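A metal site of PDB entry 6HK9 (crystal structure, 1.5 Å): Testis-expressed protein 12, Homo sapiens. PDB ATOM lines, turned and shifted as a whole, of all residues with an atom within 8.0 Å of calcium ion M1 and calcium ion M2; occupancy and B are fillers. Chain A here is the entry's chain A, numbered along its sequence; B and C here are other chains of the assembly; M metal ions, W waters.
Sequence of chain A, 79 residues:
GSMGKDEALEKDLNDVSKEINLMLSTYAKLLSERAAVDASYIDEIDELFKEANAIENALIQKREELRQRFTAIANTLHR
Calcium ion M2 is bound by water W3, water W4 and the backbone carbonyl oxygen of Glu 7 of chain A.
Calcium ion M2 has three donor atoms within binding distance.
The side-chain carboxylate of Glu 7 of chain A is in salt-bridge range of the side-chain amino group of Lys 11 (3.3 Å).
The side-chain amino group of Lys 11 lies within salt-bridge range of the side-chain carboxylate of Asp 15 (3.1 Å).
One residue has an atom within 4 Å of calcium ion M2: Glu 7 of chain A.
Calcium ion M1 is bound by water W5, at 2.2 Å.
Water W2 binds calcium ion M1.
Water W1 is bound to calcium ion M1, at 2.3 Å.
OD1 of Asp 12 is bound to calcium ion M1 (2.4 Å).
OE1 of Glu 7 of chain A is bound to calcium ion M1 (2.4 Å).
Calcium ion M1 is bound by OD2 of Asp 15, 2.4 Å away.
Calcium ion M1 has six donor atoms within binding distance.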
ATOM      1  N   ASP A   6      -8.129 -34.268 -10.849  1.00  0.00           N
ATOM      2  CA  ASP A   6      -9.026 -35.413 -10.850  1.00  0.00           C
ATOM      3  C   ASP A   6     -10.180 -35.184  -9.892  1.00  0.00           C
ATOM      4  O   ASP A   6     -11.171 -35.905  -9.917  1.00  0.00           O
ATOM      5  CB  ASP A   6      -8.283 -36.692 -10.482  1.00  0.00           C
ATOM      6  CG  ASP A   6      -7.932 -36.770  -9.021  1.00  0.00           C
ATOM      7  OD1 ASP A   6      -7.604 -35.718  -8.437  1.00  0.00           O
ATOM      8  OD2 ASP A   6      -8.002 -37.881  -8.462  1.00  0.00           O
ATOM      9  N   GLU A   7     -10.047 -34.192  -9.031  1.00  0.00           N
ATOM     10  CA  GLU A   7     -11.137 -33.742  -8.185  1.00  0.00           C
ATOM     11  C   GLU A   7     -11.780 -32.507  -8.802  1.00  0.00           C
ATOM     12  O   GLU A   7     -11.159 -31.766  -9.572  1.00  0.00           O
ATOM     13  CB  GLU A   7     -10.635 -33.457  -6.759  1.00  0.00           C
ATOM     14  CG  GLU A   7      -9.960 -34.658  -6.100  1.00  0.00           C
ATOM     15  CD  GLU A   7      -9.857 -34.535  -4.579  1.00  0.00           C
ATOM     16  OE1 GLU A   7      -9.246 -33.562  -4.090  1.00  0.00           O
ATOM     17  OE2 GLU A   7     -10.379 -35.429  -3.874  1.00  0.00           O
ATOM     18  N   ALA A   8     -13.044 -32.295  -8.458  1.00  0.00           N
ATOM     19  CA  ALA A   8     -13.782 -31.164  -9.004  1.00  0.00           C
ATOM     20  C   ALA A   8     -13.120 -29.846  -8.590  1.00  0.00           C
ATOM     21  O   ALA A   8     -12.445 -29.769  -7.577  1.00  0.00           O
ATOM     22  CB  ALA A   8     -15.232 -31.189  -8.498  1.00  0.00           C
ATOM     23  N   LEU A   9     -13.339 -28.795  -9.395  1.00  0.00           N
ATOM     24  CA  LEU A   9     -12.774 -27.484  -9.073  1.00  0.00           C
ATOM     25  C   LEU A   9     -13.260 -27.013  -7.708  1.00  0.00           C
ATOM     26  O   LEU A   9     -12.515 -26.355  -6.975  1.00  0.00           O
ATOM     27  CB  LEU A   9     -13.147 -26.470 -10.146  1.00  0.00           C
ATOM     28  CG  LEU A   9     -12.456 -26.633 -11.488  1.00  0.00           C
ATOM     29  CD1 LEU A   9     -13.094 -25.758 -12.560  1.00  0.00           C
ATOM     30  CD2 LEU A   9     -10.967 -26.318 -11.342  1.00  0.00           C
ATOM     31  N   GLU A  10     -14.509 -27.333  -7.369  1.00  0.00           N
ATOM     32  CA  GLU A  10     -15.065 -26.955  -6.061  1.00  0.00           C
ATOM     33  C   GLU A  10     -14.302 -27.629  -4.940  1.00  0.00           C
ATOM     34  O   GLU A  10     -14.099 -27.019  -3.876  1.00  0.00           O
ATOM     35  CB  GLU A  10     -16.532 -27.381  -6.003  1.00  0.00           C
ATOM     36  CG  GLU A  10     -17.443 -26.660  -6.946  1.00  0.00           C
ATOM     37  CD  GLU A  10     -17.733 -27.454  -8.229  1.00  0.00           C
ATOM     38  OE1 GLU A  10     -16.867 -28.234  -8.658  1.00  0.00           O
ATOM     39  OE2 GLU A  10     -18.834 -27.318  -8.820  1.00  0.00           O
ATOM     40  N   LYS A  11     -13.941 -28.894  -5.127  1.00  0.00           N
ATOM     41  CA  LYS A  11     -13.166 -29.616  -4.127  1.00  0.00           C
ATOM     42  C   LYS A  11     -11.771 -29.048  -4.028  1.00  0.00           C
ATOM     43  O   LYS A  11     -11.234 -28.853  -2.927  1.00  0.00           O
ATOM     44  CB  LYS A  11     -13.101 -31.095  -4.497  1.00  0.00           C
ATOM     45  CG  LYS A  11     -12.189 -31.955  -3.647  1.00  0.00           C
ATOM     46  CD  LYS A  11     -12.580 -31.910  -2.173  1.00  0.00           C
ATOM     47  CE  LYS A  11     -11.920 -33.032  -1.372  1.00  0.00           C
ATOM     48  NZ  LYS A  11     -10.437 -33.105  -1.546  1.00  0.00           N
ATOM     49  N   ASP A  12     -11.158 -28.748  -5.183  1.00  0.00           N
ATOM     50  CA  ASP A  12      -9.809 -28.218  -5.169  1.00  0.00           C
ATOM     51  C   ASP A  12      -9.779 -26.822  -4.559  1.00  0.00           C
ATOM     52  O   ASP A  12      -8.827 -26.469  -3.864  1.00  0.00           O
ATOM     53  CB  ASP A  12      -9.208 -28.233  -6.581  1.00  0.00           C
ATOM     54  CG  ASP A  12      -8.757 -29.611  -6.996  1.00  0.00           C
ATOM     55  OD1 ASP A  12      -8.677 -30.503  -6.118  1.00  0.00           O
ATOM     56  OD2 ASP A  12      -8.507 -29.833  -8.216  1.00  0.00           O
ATOM     57  N   LEU A  13     -10.807 -26.025  -4.793  1.00  0.00           N
ATOM     58  CA  LEU A  13     -10.880 -24.714  -4.155  1.00  0.00           C
ATOM     59  C   LEU A  13     -10.927 -24.844  -2.642  1.00  0.00           C
ATOM     60  O   LEU A  13     -10.341 -24.035  -1.913  1.00  0.00           O
ATOM     61  CB  LEU A  13     -12.097 -23.947  -4.657  1.00  0.00           C
ATOM     62  CG  LEU A  13     -12.218 -22.536  -4.081  1.00  0.00           C
ATOM     63  CD1 LEU A  13     -10.935 -21.729  -4.305  1.00  0.00           C
ATOM     64  CD2 LEU A  13     -13.421 -21.859  -4.718  1.00  0.00           C
ATOM     65  N   ASN A  14     -11.643 -25.847  -2.141  1.00  0.00           N
ATOM     66  CA  ASN A  14     -11.747 -26.042  -0.706  1.00  0.00           C
ATOM     67  C   ASN A  14     -10.431 -26.565  -0.147  1.00  0.00           C
ATOM     68  O   ASN A  14     -10.031 -26.178   0.970  1.00  0.00           O
ATOM     69  CB  ASN A  14     -12.883 -27.006  -0.407  1.00  0.00           C
ATOM     70  CG  ASN A  14     -13.298 -26.960   1.047  1.00  0.00           C
ATOM     71  OD1 ASN A  14     -12.952 -27.852   1.830  1.00  0.00           O
ATOM     72  ND2 ASN A  14     -14.023 -25.908   1.427  1.00  0.00           N
ATOM     73  N   ASP A  15      -9.724 -27.406  -0.900  1.00  0.00           N
ATOM     74  CA  ASP A  15      -8.417 -27.867  -0.425  1.00  0.00           C
ATOM     75  C   ASP A  15      -7.429 -26.718  -0.298  1.00  0.00           C
ATOM     76  O   ASP A  15      -6.696 -26.617   0.694  1.00  0.00           O
ATOM     77  CB  ASP A  15      -7.841 -28.898  -1.384  1.00  0.00           C
ATOM     78  CG  ASP A  15      -8.646 -30.179  -1.435  1.00  0.00           C
ATOM     79  OD1 ASP A  15      -9.271 -30.526  -0.407  1.00  0.00           O
ATOM     80  OD2 ASP A  15      -8.633 -30.832  -2.500  1.00  0.00           O
ATOM     81  N   VAL A  16      -7.335 -25.863  -1.311  1.00  0.00           N
ATOM     82  CA  VAL A  16      -6.345 -24.799  -1.256  1.00  0.00           C
ATOM     83  C   VAL A  16      -6.722 -23.786  -0.178  1.00  0.00           C
ATOM     84  O   VAL A  16      -5.841 -23.202   0.483  1.00  0.00           O
ATOM     85  CB  VAL A  16      -6.139 -24.132  -2.632  1.00  0.00           C
ATOM     86  CG1 VAL A  16      -7.403 -23.417  -3.056  1.00  0.00           C
ATOM     87  CG2 VAL A  16      -4.957 -23.164  -2.550  1.00  0.00           C
ATOM     88  N   GLU A  19      -5.248 -24.992   2.942  1.00  0.00           N
ATOM     89  CA  GLU A  19      -3.817 -24.742   2.968  1.00  0.00           C
ATOM     90  C   GLU A  19      -3.517 -23.300   3.336  1.00  0.00           C
ATOM     91  O   GLU A  19      -2.608 -23.029   4.116  1.00  0.00           O
ATOM     92  CB  GLU A  19      -3.194 -25.039   1.611  1.00  0.00           C
ATOM     93  CG  GLU A  19      -3.096 -26.505   1.219  1.00  0.00           C
ATOM     94  CD  GLU A  19      -2.129 -26.709   0.043  1.00  0.00           C
ATOM     95  OE1 GLU A  19      -0.887 -26.764   0.302  1.00  0.00           O
ATOM     96  OE2 GLU A  19      -2.612 -26.773  -1.113  1.00  0.00           O
ATOM     97  N   ASP B   6      -6.467 -31.908 -13.279  1.00  0.00           N
ATOM     98  CA  ASP B   6      -6.748 -31.223 -14.531  1.00  0.00           C
ATOM     99  C   ASP B   6      -5.634 -31.467 -15.532  1.00  0.00           C
ATOM    100  O   ASP B   6      -5.781 -31.192 -16.717  1.00  0.00           O
ATOM    101  CB  ASP B   6      -6.935 -29.727 -14.308  1.00  0.00           C
ATOM    102  CG  ASP B   6      -5.644 -29.008 -14.024  1.00  0.00           C
ATOM    103  OD1 ASP B   6      -4.781 -29.595 -13.341  1.00  0.00           O
ATOM    104  OD2 ASP B   6      -5.495 -27.866 -14.498  1.00  0.00           O
ATOM    105  N   GLU B   7      -4.505 -31.978 -15.056  1.00  0.00           N
ATOM    106  CA  GLU B   7      -3.432 -32.424 -15.915  1.00  0.00           C
ATOM    107  C   GLU B   7      -3.504 -33.938 -16.059  1.00  0.00           C
ATOM    108  O   GLU B   7      -4.045 -34.648 -15.203  1.00  0.00           O
ATOM    109  CB  GLU B   7      -2.068 -31.979 -15.357  1.00  0.00           C
ATOM    110  CG  GLU B   7      -1.949 -30.468 -15.171  1.00  0.00           C
ATOM    111  CD  GLU B   7      -0.504 -29.987 -15.045  1.00  0.00           C
ATOM    112  OE1 GLU B   7       0.209 -30.443 -14.127  1.00  0.00           O
ATOM    113  OE2 GLU B   7      -0.084 -29.143 -15.863  1.00  0.00           O
ATOM    114  N   GLU C  51      -2.983 -19.779  -6.828  1.00  0.00           N
ATOM    115  CA  GLU C  51      -3.611 -21.051  -7.150  1.00  0.00           C
ATOM    116  C   GLU C  51      -5.097 -21.025  -6.785  1.00  0.00           C
ATOM    117  O   GLU C  51      -5.944 -21.486  -7.566  1.00  0.00           O
ATOM    118  CB  GLU C  51      -2.901 -22.185  -6.406  1.00  0.00           C
ATOM    119  CG  GLU C  51      -3.733 -23.435  -6.330  1.00  0.00           C
ATOM    120  CD  GLU C  51      -2.941 -24.683  -5.976  1.00  0.00           C
ATOM    121  OE1 GLU C  51      -1.940 -24.569  -5.241  1.00  0.00           O
ATOM    122  OE2 GLU C  51      -3.360 -25.773  -6.433  1.00  0.00           O
ATOM    123  N   ILE C  55      -8.284 -21.469  -9.408  1.00  0.00           N
ATOM    124  CA  ILE C  55      -9.343 -22.455  -9.230  1.00  0.00           C
ATOM    125  C   ILE C  55     -10.698 -21.771  -9.130  1.00  0.00           C
ATOM    126  O   ILE C  55     -11.689 -22.216  -9.726  1.00  0.00           O
ATOM    127  CB  ILE C  55      -9.077 -23.330  -7.993  1.00  0.00           C
ATOM    128  CG1 ILE C  55      -7.771 -24.120  -8.149  1.00  0.00           C
ATOM    129  CG2 ILE C  55     -10.248 -24.265  -7.756  1.00  0.00           C
ATOM    130  CD1 ILE C  55      -7.306 -24.732  -6.855  1.00  0.00           C
ATOM    131  N   LYS C  62     -16.887 -22.806 -14.980  1.00  0.00           N
ATOM    132  CA  LYS C  62     -17.555 -24.107 -15.054  1.00  0.00           C
ATOM    133  C   LYS C  62     -19.054 -23.955 -14.864  1.00  0.00           C
ATOM    134  O   LYS C  62     -19.858 -24.583 -15.584  1.00  0.00           O
ATOM    135  CB  LYS C  62     -16.993 -25.002 -13.961  1.00  0.00           C
ATOM    136  CG  LYS C  62     -17.836 -26.258 -13.715  1.00  0.00           C
ATOM    137  CD  LYS C  62     -17.226 -27.101 -12.615  1.00  0.00           C
ATOM    138  CE  LYS C  62     -18.109 -28.277 -12.262  1.00  0.00           C
ATOM    139  NZ  LYS C  62     -17.453 -29.123 -11.233  1.00  0.00           N
HETATM  140 CA    CA M   1      -7.632 -31.835  -4.438  1.00  0.00          CA
HETATM  141 CA    CA M   2     -10.504 -31.018 -11.927  1.00  0.00          CA
HETATM  142 CA    CA M   3      -6.064 -35.928 -14.298  1.00  0.00          CA
HETATM  143  O   HOH W   1      -6.593 -33.061  -6.087  1.00  0.00           O
HETATM  144  O   HOH W   2      -6.170 -30.140  -4.374  1.00  0.00           O
HETATM  145  O   HOH W   3      -8.636 -32.274 -11.830  1.00  0.00           O
HETATM  146  O   HOH W   4      -9.376 -29.480 -10.554  1.00  0.00           O
HETATM  147  O   HOH W   5      -6.017 -32.675  -3.190  1.00  0.00           O
